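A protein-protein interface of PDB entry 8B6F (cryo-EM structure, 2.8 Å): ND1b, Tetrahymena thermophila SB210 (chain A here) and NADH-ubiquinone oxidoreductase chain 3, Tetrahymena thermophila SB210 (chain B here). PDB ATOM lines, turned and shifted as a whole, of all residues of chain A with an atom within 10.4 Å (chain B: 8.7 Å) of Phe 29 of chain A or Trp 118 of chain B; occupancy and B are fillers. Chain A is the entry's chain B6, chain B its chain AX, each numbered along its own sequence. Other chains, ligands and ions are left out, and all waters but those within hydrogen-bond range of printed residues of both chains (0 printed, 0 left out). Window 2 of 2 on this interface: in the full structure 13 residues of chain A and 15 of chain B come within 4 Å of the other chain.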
ATOM      1  N   ARG A  26     -22.333   0.582  25.727  1.00  0.00           N
ATOM      2  CA  ARG A  26     -22.960   0.634  24.415  1.00  0.00           C
ATOM      3  C   ARG A  26     -22.411   1.811  23.617  1.00  0.00           C
ATOM      4  O   ARG A  26     -22.213   2.903  24.159  1.00  0.00           O
ATOM      5  CB  ARG A  26     -24.482   0.745  24.539  1.00  0.00           C
ATOM      6  CG  ARG A  26     -25.196   0.904  23.210  1.00  0.00           C
ATOM      7  CD  ARG A  26     -26.695   0.685  23.342  1.00  0.00           C
ATOM      8  NE  ARG A  26     -27.284   1.467  24.424  1.00  0.00           N
ATOM      9  CZ  ARG A  26     -27.569   0.996  25.633  1.00  0.00           C
ATOM     10  NH1 ARG A  26     -27.331  -0.263  25.962  1.00  0.00           N
ATOM     11  NH2 ARG A  26     -28.108   1.812  26.534  1.00  0.00           N
ATOM     12  N   TYR A  27     -22.162   1.578  22.331  1.00  0.00           N
ATOM     13  CA  TYR A  27     -21.641   2.598  21.434  1.00  0.00           C
ATOM     14  C   TYR A  27     -22.755   3.537  20.973  1.00  0.00           C
ATOM     15  O   TYR A  27     -23.944   3.288  21.177  1.00  0.00           O
ATOM     16  CB  TYR A  27     -20.986   1.953  20.210  1.00  0.00           C
ATOM     17  CG  TYR A  27     -19.478   2.032  20.173  1.00  0.00           C
ATOM     18  CD1 TYR A  27     -18.825   3.257  20.197  1.00  0.00           C
ATOM     19  CD2 TYR A  27     -18.710   0.882  20.071  1.00  0.00           C
ATOM     20  CE1 TYR A  27     -17.447   3.330  20.150  1.00  0.00           C
ATOM     21  CE2 TYR A  27     -17.334   0.944  20.024  1.00  0.00           C
ATOM     22  CZ  TYR A  27     -16.709   2.170  20.063  1.00  0.00           C
ATOM     23  OH  TYR A  27     -15.335   2.237  20.013  1.00  0.00           O
ATOM     24  N   ARG A  28     -22.350   4.632  20.339  1.00  0.00           N
ATOM     25  CA  ARG A  28     -23.252   5.473  19.566  1.00  0.00           C
ATOM     26  C   ARG A  28     -23.184   5.064  18.101  1.00  0.00           C
ATOM     27  O   ARG A  28     -22.133   4.652  17.604  1.00  0.00           O
ATOM     28  CB  ARG A  28     -22.898   6.955  19.701  1.00  0.00           C
ATOM     29  CG  ARG A  28     -23.101   7.535  21.086  1.00  0.00           C
ATOM     30  CD  ARG A  28     -23.376   9.032  21.013  1.00  0.00           C
ATOM     31  NE  ARG A  28     -22.404   9.748  20.195  1.00  0.00           N
ATOM     32  CZ  ARG A  28     -21.310  10.340  20.655  1.00  0.00           C
ATOM     33  NH1 ARG A  28     -20.991  10.304  21.938  1.00  0.00           N
ATOM     34  NH2 ARG A  28     -20.518  10.987  19.807  1.00  0.00           N
ATOM     35  N   PHE A  29     -24.317   5.177  17.406  1.00  0.00           N
ATOM     36  CA  PHE A  29     -24.349   4.758  16.009  1.00  0.00           C
ATOM     37  C   PHE A  29     -23.399   5.598  15.163  1.00  0.00           C
ATOM     38  O   PHE A  29     -22.687   5.063  14.306  1.00  0.00           O
ATOM     39  CB  PHE A  29     -25.779   4.820  15.457  1.00  0.00           C
ATOM     40  CG  PHE A  29     -26.465   6.141  15.657  1.00  0.00           C
ATOM     41  CD1 PHE A  29     -26.322   7.161  14.733  1.00  0.00           C
ATOM     42  CD2 PHE A  29     -27.289   6.345  16.750  1.00  0.00           C
ATOM     43  CE1 PHE A  29     -26.965   8.368  14.910  1.00  0.00           C
ATOM     44  CE2 PHE A  29     -27.933   7.549  16.932  1.00  0.00           C
ATOM     45  CZ  PHE A  29     -27.771   8.563  16.011  1.00  0.00           C
ATOM     46  N   ASP A  30     -23.381   6.915  15.378  1.00  0.00           N
ATOM     47  CA  ASP A  30     -22.470   7.765  14.618  1.00  0.00           C
ATOM     48  C   ASP A  30     -21.016   7.441  14.940  1.00  0.00           C
ATOM     49  O   ASP A  30     -20.173   7.380  14.039  1.00  0.00           O
ATOM     50  CB  ASP A  30     -22.762   9.236  14.898  1.00  0.00           C
ATOM     51  CG  ASP A  30     -22.537   9.603  16.345  1.00  0.00           C
ATOM     52  OD1 ASP A  30     -22.923   8.805  17.223  1.00  0.00           O
ATOM     53  OD2 ASP A  30     -21.965  10.681  16.609  1.00  0.00           O
ATOM     54  N   GLN A  31     -20.701   7.241  16.221  1.00  0.00           N
ATOM     55  CA  GLN A  31     -19.332   6.911  16.603  1.00  0.00           C
ATOM     56  C   GLN A  31     -18.869   5.625  15.933  1.00  0.00           C
ATOM     57  O   GLN A  31     -17.781   5.573  15.349  1.00  0.00           O
ATOM     58  CB  GLN A  31     -19.226   6.782  18.122  1.00  0.00           C
ATOM     59  CG  GLN A  31     -19.258   8.102  18.857  1.00  0.00           C
ATOM     60  CD  GLN A  31     -19.085   7.927  20.348  1.00  0.00           C
ATOM     61  OE1 GLN A  31     -19.382   6.866  20.896  1.00  0.00           O
ATOM     62  NE2 GLN A  31     -18.591   8.964  21.011  1.00  0.00           N
ATOM     63  N   PHE A  32     -19.685   4.575  16.002  1.00  0.00           N
ATOM     64  CA  PHE A  32     -19.281   3.307  15.409  1.00  0.00           C
ATOM     65  C   PHE A  32     -19.178   3.412  13.896  1.00  0.00           C
ATOM     66  O   PHE A  32     -18.273   2.832  13.287  1.00  0.00           O
ATOM     67  CB  PHE A  32     -20.254   2.197  15.787  1.00  0.00           C
ATOM     68  CG  PHE A  32     -20.015   0.927  15.035  1.00  0.00           C
ATOM     69  CD1 PHE A  32     -18.827   0.235  15.186  1.00  0.00           C
ATOM     70  CD2 PHE A  32     -20.964   0.441  14.153  1.00  0.00           C
ATOM     71  CE1 PHE A  32     -18.595  -0.929  14.484  1.00  0.00           C
ATOM     72  CE2 PHE A  32     -20.739  -0.721  13.448  1.00  0.00           C
ATOM     73  CZ  PHE A  32     -19.552  -1.408  13.614  1.00  0.00           C
ATOM     74  N   THR A  33     -20.099   4.140  13.270  1.00  0.00           N
ATOM     75  CA  THR A  33     -20.041   4.291  11.824  1.00  0.00           C
ATOM     76  C   THR A  33     -18.770   5.012  11.403  1.00  0.00           C
ATOM     77  O   THR A  33     -18.103   4.603  10.447  1.00  0.00           O
ATOM     78  CB  THR A  33     -21.272   5.043  11.334  1.00  0.00           C
ATOM     79  OG1 THR A  33     -22.454   4.444  11.880  1.00  0.00           O
ATOM     80  CG2 THR A  33     -21.348   4.989   9.841  1.00  0.00           C
ATOM     81  N   GLN A  34     -18.416   6.087  12.107  1.00  0.00           N
ATOM     82  CA  GLN A  34     -17.177   6.789  11.793  1.00  0.00           C
ATOM     83  C   GLN A  34     -15.978   5.868  11.978  1.00  0.00           C
ATOM     84  O   GLN A  34     -15.109   5.777  11.106  1.00  0.00           O
ATOM     85  CB  GLN A  34     -17.044   8.037  12.664  1.00  0.00           C
ATOM     86  CG  GLN A  34     -18.071   9.106  12.348  1.00  0.00           C
ATOM     87  CD  GLN A  34     -17.992  10.281  13.296  1.00  0.00           C
ATOM     88  OE1 GLN A  34     -17.123  10.335  14.164  1.00  0.00           O
ATOM     89  NE2 GLN A  34     -18.903  11.234  13.133  1.00  0.00           N
ATOM     90  N   LEU A  35     -15.914   5.175  13.117  1.00  0.00           N
ATOM     91  CA  LEU A  35     -14.815   4.247  13.350  1.00  0.00           C
ATOM     92  C   LEU A  35     -14.713   3.242  12.214  1.00  0.00           C
ATOM     93  O   LEU A  35     -13.637   3.037  11.641  1.00  0.00           O
ATOM     94  CB  LEU A  35     -15.013   3.520  14.680  1.00  0.00           C
ATOM     95  CG  LEU A  35     -14.858   4.343  15.958  1.00  0.00           C
ATOM     96  CD1 LEU A  35     -15.219   3.511  17.174  1.00  0.00           C
ATOM     97  CD2 LEU A  35     -13.440   4.880  16.084  1.00  0.00           C
ATOM     98  N   ASN A  36     -15.831   2.601  11.877  1.00  0.00           N
ATOM     99  CA  ASN A  36     -15.824   1.600  10.820  1.00  0.00           C
ATOM    100  C   ASN A  36     -15.291   2.190   9.518  1.00  0.00           C
ATOM    101  O   ASN A  36     -14.244   1.774   9.012  1.00  0.00           O
ATOM    102  CB  ASN A  36     -17.237   1.044  10.641  1.00  0.00           C
ATOM    103  CG  ASN A  36     -17.296  -0.108   9.666  1.00  0.00           C
ATOM    104  OD1 ASN A  36     -16.269  -0.601   9.206  1.00  0.00           O
ATOM    105  ND2 ASN A  36     -18.503  -0.566   9.371  1.00  0.00           N
ATOM    106  N   TRP A  37     -16.011   3.163   8.959  1.00  0.00           N
ATOM    107  CA  TRP A  37     -15.701   3.665   7.628  1.00  0.00           C
ATOM    108  C   TRP A  37     -14.385   4.429   7.554  1.00  0.00           C
ATOM    109  O   TRP A  37     -13.923   4.707   6.443  1.00  0.00           O
ATOM    110  CB  TRP A  37     -16.836   4.567   7.142  1.00  0.00           C
ATOM    111  CG  TRP A  37     -18.087   3.824   6.814  1.00  0.00           C
ATOM    112  CD1 TRP A  37     -19.015   3.351   7.694  1.00  0.00           C
ATOM    113  CD2 TRP A  37     -18.552   3.467   5.509  1.00  0.00           C
ATOM    114  NE1 TRP A  37     -20.030   2.721   7.017  1.00  0.00           N
ATOM    115  CE2 TRP A  37     -19.770   2.782   5.673  1.00  0.00           C
ATOM    116  CE3 TRP A  37     -18.056   3.665   4.217  1.00  0.00           C
ATOM    117  CZ2 TRP A  37     -20.497   2.287   4.593  1.00  0.00           C
ATOM    118  CZ3 TRP A  37     -18.780   3.175   3.146  1.00  0.00           C
ATOM    119  CH2 TRP A  37     -19.988   2.494   3.341  1.00  0.00           C
ATOM    120  N   LYS A  38     -13.772   4.777   8.685  1.00  0.00           N
ATOM    121  CA  LYS A  38     -12.495   5.481   8.663  1.00  0.00           C
ATOM    122  C   LYS A  38     -11.302   4.595   8.981  1.00  0.00           C
ATOM    123  O   LYS A  38     -10.199   4.875   8.500  1.00  0.00           O
ATOM    124  CB  LYS A  38     -12.515   6.648   9.656  1.00  0.00           C
ATOM    125  CG  LYS A  38     -13.520   7.734   9.313  1.00  0.00           C
ATOM    126  CD  LYS A  38     -13.514   8.835  10.361  1.00  0.00           C
ATOM    127  CE  LYS A  38     -14.597   9.865  10.091  1.00  0.00           C
ATOM    128  NZ  LYS A  38     -14.402  10.558   8.790  1.00  0.00           N
ATOM    129  N   ASN B  58     -34.658  13.144   9.890  1.00  0.00           N
ATOM    130  CA  ASN B  58     -33.636  13.844   9.126  1.00  0.00           C
ATOM    131  C   ASN B  58     -32.605  12.829   8.651  1.00  0.00           C
ATOM    132  O   ASN B  58     -31.957  12.166   9.468  1.00  0.00           O
ATOM    133  CB  ASN B  58     -32.975  14.932   9.969  1.00  0.00           C
ATOM    134  CG  ASN B  58     -32.084  15.840   9.151  1.00  0.00           C
ATOM    135  OD1 ASN B  58     -32.127  15.828   7.922  1.00  0.00           O
ATOM    136  ND2 ASN B  58     -31.272  16.640   9.830  1.00  0.00           N
ATOM    137  N   PHE B  59     -32.465  12.705   7.335  1.00  0.00           N
ATOM    138  CA  PHE B  59     -31.541  11.750   6.732  1.00  0.00           C
ATOM    139  C   PHE B  59     -30.245  12.472   6.368  1.00  0.00           C
ATOM    140  O   PHE B  59     -29.891  12.645   5.203  1.00  0.00           O
ATOM    141  CB  PHE B  59     -32.193  11.098   5.514  1.00  0.00           C
ATOM    142  CG  PHE B  59     -31.462   9.895   4.979  1.00  0.00           C
ATOM    143  CD1 PHE B  59     -30.429   9.299   5.685  1.00  0.00           C
ATOM    144  CD2 PHE B  59     -31.820   9.363   3.752  1.00  0.00           C
ATOM    145  CE1 PHE B  59     -29.773   8.196   5.175  1.00  0.00           C
ATOM    146  CE2 PHE B  59     -31.170   8.261   3.240  1.00  0.00           C
ATOM    147  CZ  PHE B  59     -30.145   7.676   3.951  1.00  0.00           C
ATOM    148  N   ASN B  60     -29.536  12.902   7.408  1.00  0.00           N
ATOM    149  CA  ASN B  60     -28.307  13.669   7.251  1.00  0.00           C
ATOM    150  C   ASN B  60     -27.070  12.787   7.147  1.00  0.00           C
ATOM    151  O   ASN B  60     -25.952  13.311   7.117  1.00  0.00           O
ATOM    152  CB  ASN B  60     -28.149  14.661   8.407  1.00  0.00           C
ATOM    153  CG  ASN B  60     -28.234  13.998   9.761  1.00  0.00           C
ATOM    154  OD1 ASN B  60     -28.114  12.780   9.877  1.00  0.00           O
ATOM    155  ND2 ASN B  60     -28.446  14.799  10.798  1.00  0.00           N
ATOM    156  N   PHE B  61     -27.242  11.467   7.096  1.00  0.00           N
ATOM    157  CA  PHE B  61     -26.140  10.532   6.896  1.00  0.00           C
ATOM    158  C   PHE B  61     -26.309   9.763   5.589  1.00  0.00           C
ATOM    159  O   PHE B  61     -25.859   8.623   5.467  1.00  0.00           O
ATOM    160  CB  PHE B  61     -26.029   9.568   8.076  1.00  0.00           C
ATOM    161  CG  PHE B  61     -27.262   8.743   8.305  1.00  0.00           C
ATOM    162  CD1 PHE B  61     -28.289   9.220   9.102  1.00  0.00           C
ATOM    163  CD2 PHE B  61     -27.391   7.488   7.735  1.00  0.00           C
ATOM    164  CE1 PHE B  61     -29.424   8.465   9.318  1.00  0.00           C
ATOM    165  CE2 PHE B  61     -28.523   6.727   7.949  1.00  0.00           C
ATOM    166  CZ  PHE B  61     -29.541   7.217   8.742  1.00  0.00           C
ATOM    167  N   PHE B  62     -26.951  10.385   4.598  1.00  0.00           N
ATOM    168  CA  PHE B  62     -27.253   9.699   3.349  1.00  0.00           C
ATOM    169  C   PHE B  62     -26.011   9.397   2.524  1.00  0.00           C
ATOM    170  O   PHE B  62     -26.056   8.506   1.670  1.00  0.00           O
ATOM    171  CB  PHE B  62     -28.231  10.527   2.513  1.00  0.00           C
ATOM    172  CG  PHE B  62     -27.691  11.862   2.084  1.00  0.00           C
ATOM    173  CD1 PHE B  62     -27.018  11.993   0.880  1.00  0.00           C
ATOM    174  CD2 PHE B  62     -27.880  12.987   2.865  1.00  0.00           C
ATOM    175  CE1 PHE B  62     -26.528  13.217   0.475  1.00  0.00           C
ATOM    176  CE2 PHE B  62     -27.394  14.216   2.465  1.00  0.00           C
ATOM    177  CZ  PHE B  62     -26.717  14.331   1.268  1.00  0.00           C
ATOM    178  N   MET B  63     -24.905  10.107   2.751  1.00  0.00           N
ATOM    179  CA  MET B  63     -23.685   9.809   2.011  1.00  0.00           C
ATOM    180  C   MET B  63     -23.184   8.405   2.311  1.00  0.00           C
ATOM    181  O   MET B  63     -22.602   7.752   1.437  1.00  0.00           O
ATOM    182  CB  MET B  63     -22.602  10.833   2.343  1.00  0.00           C
ATOM    183  CG  MET B  63     -22.924  12.246   1.889  1.00  0.00           C
ATOM    184  SD  MET B  63     -23.280  12.370   0.125  1.00  0.00           S
ATOM    185  CE  MET B  63     -21.799  11.662  -0.586  1.00  0.00           C
ATOM    186  N   LEU B  64     -23.400   7.925   3.533  1.00  0.00           N
ATOM    187  CA  LEU B  64     -22.985   6.571   3.874  1.00  0.00           C
ATOM    188  C   LEU B  64     -23.733   5.541   3.041  1.00  0.00           C
ATOM    189  O   LEU B  64     -23.134   4.580   2.544  1.00  0.00           O
ATOM    190  CB  LEU B  64     -23.210   6.333   5.361  1.00  0.00           C
ATOM    191  CG  LEU B  64     -22.383   7.254   6.256  1.00  0.00           C
ATOM    192  CD1 LEU B  64     -22.883   7.108   7.653  1.00  0.00           C
ATOM    193  CD2 LEU B  64     -20.899   6.934   6.178  1.00  0.00           C
ATOM    194  N   ASN B 114     -14.445  14.509   4.065  1.00  0.00           N
ATOM    195  CA  ASN B 114     -15.197  14.489   5.319  1.00  0.00           C
ATOM    196  C   ASN B 114     -16.696  14.356   5.061  1.00  0.00           C
ATOM    197  O   ASN B 114     -17.516  15.082   5.624  1.00  0.00           O
ATOM    198  CB  ASN B 114     -14.899  15.733   6.158  1.00  0.00           C
ATOM    199  CG  ASN B 114     -13.425  15.885   6.470  1.00  0.00           C
ATOM    200  OD1 ASN B 114     -12.835  16.939   6.239  1.00  0.00           O
ATOM    201  ND2 ASN B 114     -12.819  14.825   6.994  1.00  0.00           N
ATOM    202  N   VAL B 115     -17.049  13.407   4.193  1.00  0.00           N
ATOM    203  CA  VAL B 115     -18.445  13.111   3.896  1.00  0.00           C
ATOM    204  C   VAL B 115     -18.936  11.874   4.628  1.00  0.00           C
ATOM    205  O   VAL B 115     -20.076  11.445   4.411  1.00  0.00           O
ATOM    206  CB  VAL B 115     -18.669  12.949   2.377  1.00  0.00           C
ATOM    207  CG1 VAL B 115     -18.530  14.289   1.678  1.00  0.00           C
ATOM    208  CG2 VAL B 115     -17.689  11.943   1.790  1.00  0.00           C
ATOM    209  N   LEU B 116     -18.111  11.290   5.498  1.00  0.00           N
ATOM    210  CA  LEU B 116     -18.453  10.084   6.242  1.00  0.00           C
ATOM    211  C   LEU B 116     -18.902  10.394   7.665  1.00  0.00           C
ATOM    212  O   LEU B 116     -18.740   9.560   8.561  1.00  0.00           O
ATOM    213  CB  LEU B 116     -17.263   9.125   6.260  1.00  0.00           C
ATOM    214  CG  LEU B 116     -16.677   8.738   4.900  1.00  0.00           C
ATOM    215  CD1 LEU B 116     -15.430   7.892   5.079  1.00  0.00           C
ATOM    216  CD2 LEU B 116     -17.705   8.000   4.058  1.00  0.00           C
ATOM    217  N   SER B 117     -19.458  11.581   7.895  1.00  0.00           N
ATOM    218  CA  SER B 117     -19.877  11.995   9.224  1.00  0.00           C
ATOM    219  C   SER B 117     -21.185  12.767   9.124  1.00  0.00           C
ATOM    220  O   SER B 117     -21.555  13.271   8.062  1.00  0.00           O
ATOM    221  CB  SER B 117     -18.807  12.854   9.910  1.00  0.00           C
ATOM    222  OG  SER B 117     -18.516  14.012   9.146  1.00  0.00           O
ATOM    223  N   TRP B 118     -21.881  12.853  10.256  1.00  0.00           N
ATOM    224  CA  TRP B 118     -23.144  13.576  10.304  1.00  0.00           C
ATOM    225  C   TRP B 118     -22.922  15.059  10.037  1.00  0.00           C
ATOM    226  O   TRP B 118     -21.913  15.640  10.448  1.00  0.00           O
ATOM    227  CB  TRP B 118     -23.806  13.379  11.669  1.00  0.00           C
ATOM    228  CG  TRP B 118     -24.682  12.168  11.741  1.00  0.00           C
ATOM    229  CD1 TRP B 118     -26.024  12.146  11.980  1.00  0.00           C
ATOM    230  CD2 TRP B 118     -24.283  10.803  11.566  1.00  0.00           C
ATOM    231  NE1 TRP B 118     -26.485  10.852  11.969  1.00  0.00           N
ATOM    232  CE2 TRP B 118     -25.435  10.009  11.715  1.00  0.00           C
ATOM    233  CE3 TRP B 118     -23.062  10.176  11.298  1.00  0.00           C
ATOM    234  CZ2 TRP B 118     -25.405   8.620  11.606  1.00  0.00           C
ATOM    235  CZ3 TRP B 118     -23.033   8.798  11.188  1.00  0.00           C
ATOM    236  CH2 TRP B 118     -24.198   8.034  11.342  1.00  0.00           C
ATOM    237  N   SER B 119     -23.873  15.671   9.339  1.00  0.00           N
ATOM    238  CA  SER B 119     -23.811  17.074   8.965  1.00  0.00           C
ATOM    239  C   SER B 119     -25.006  17.817   9.547  1.00  0.00           C
ATOM    240  O   SER B 119     -25.949  17.218  10.067  1.00  0.00           O
ATOM    241  CB  SER B 119     -23.771  17.235   7.440  1.00  0.00           C
ATOM    242  OG  SER B 119     -24.904  16.639   6.833  1.00  0.00           O
ATOM    243  N   ALA B 120     -24.954  19.148   9.450  1.00  0.00           N
ATOM    244  CA  ALA B 120     -26.009  19.972  10.033  1.00  0.00           C
ATOM    245  C   ALA B 120     -27.364  19.659   9.413  1.00  0.00           C
ATOM    246  O   ALA B 120     -28.373  19.570  10.122  1.00  0.00           O
ATOM    247  CB  ALA B 120     -25.672  21.452   9.857  1.00  0.00           C
ATOM    248  N   GLU B 121     -27.411  19.496   8.095  1.00  0.00           N
ATOM    249  CA  GLU B 121     -28.655  19.164   7.411  1.00  0.00           C
ATOM    250  C   GLU B 121     -28.408  18.124   6.326  1.00  0.00           C
ATOM    251  O   GLU B 121     -29.265  17.283   6.051  1.00  0.00           O
ATOM    252  CB  GLU B 121     -29.287  20.420   6.805  1.00  0.00           C
ATOM    253  CG  GLU B 121     -30.679  20.198   6.228  1.00  0.00           C
ATOM    254  CD  GLU B 121     -31.714  19.888   7.293  1.00  0.00           C
ATOM    255  OE1 GLU B 121     -31.373  19.953   8.492  1.00  0.00           O
ATOM    256  OE2 GLU B 121     -32.869  19.583   6.930  1.00  0.00           O
ATOM    257  OXT GLU B 121     -27.348  18.095   5.701  1.00  0.00           O
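The side-chain carboxylate of Asp 30 of chain A is in salt-bridge range of the guanidinium group of Arg 28 of chain A, 3.2 Å away.
The indole nitrogen (NE1) of Trp 118 of chain B lies close to the side-chain amide oxygen (OD1) of Asn 60 of chain B (3.3 Å).
The backbone carbonyl oxygen (O) of Phe 29 of chain A lies within hydrogen-bond range of the side-chain hydroxyl (OG1) of Thr 33 of chain A, at 2.5 Å.
Phe 29 of chain A touches just one residue of chain B: Trp 118 (3.6 Å).
Printed residues of chain B within 4 Å of Asp 30 of chain A: Trp 118 (3.6 Å).
Of the printed residues of chain B, Gln 34 of chain A touches Leu 116 (3.9 Å) and Ser 117 (3.6 Å).
Of the printed residues of chain B, Trp 37 of chain A touches Leu 64 (3.9 Å) and Leu 116 (3.8 Å).
Asn 60 of chain B touches none of the printed residues of chain A.
No residue of chain A comes within 4 Å of Phe 61 of chain B.
Of the printed residues of chain A, Leu 64 of chain B touches Thr 33 and Trp 37.
Printed residues of chain A within 4 Å of Leu 116 of chain B: Gln 34 and Trp 37.
Of chain A, only Gln 34 (3.6 Å) comes within 4 Å of Ser 117 of chain B.
Of chain A, only Phe 29 and Asp 30 come within 4 Å of Trp 118 of chain B.
The nearest residue of chain B that does not touch Phe 29 of chain A is Phe 61 of chain B (6.0 Å).
The nearest residue of chain A that does not touch Trp 118 of chain B is Thr 33 of chain A (4.03 Å).
Of the 15 printed residues of chain B, 4 touch a printed residue of chain A.
Hydrophobic or aromatic side chains of chain B within 4 Å of the printed part of chain A: Leu 64, Leu 116 and Trp 118.
Hydrophobic or aromatic side chains of chain A within 4 Å of the printed part of chain B: Phe 29 and Trp 37.
Among the printed residues, no Asp or Glu carboxylate lies within 4 Å of a Lys or Arg side-chain nitrogen of the other chain.
Among the printed residues, merely in contact across the chains: Phe 29 of chain A with Trp 118 of chain B, Asp 30 of chain A with Trp 118 of chain B, Thr 33 of chain A with Leu 64 of chain B, Gln 34 of chain A with Leu 116 of chain B, Gln 34 of chain A with Ser 117 of chain B, Trp 37 of chain A with Leu 64 of chain B and Trp 37 of chain A with Leu 116 of chain B.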
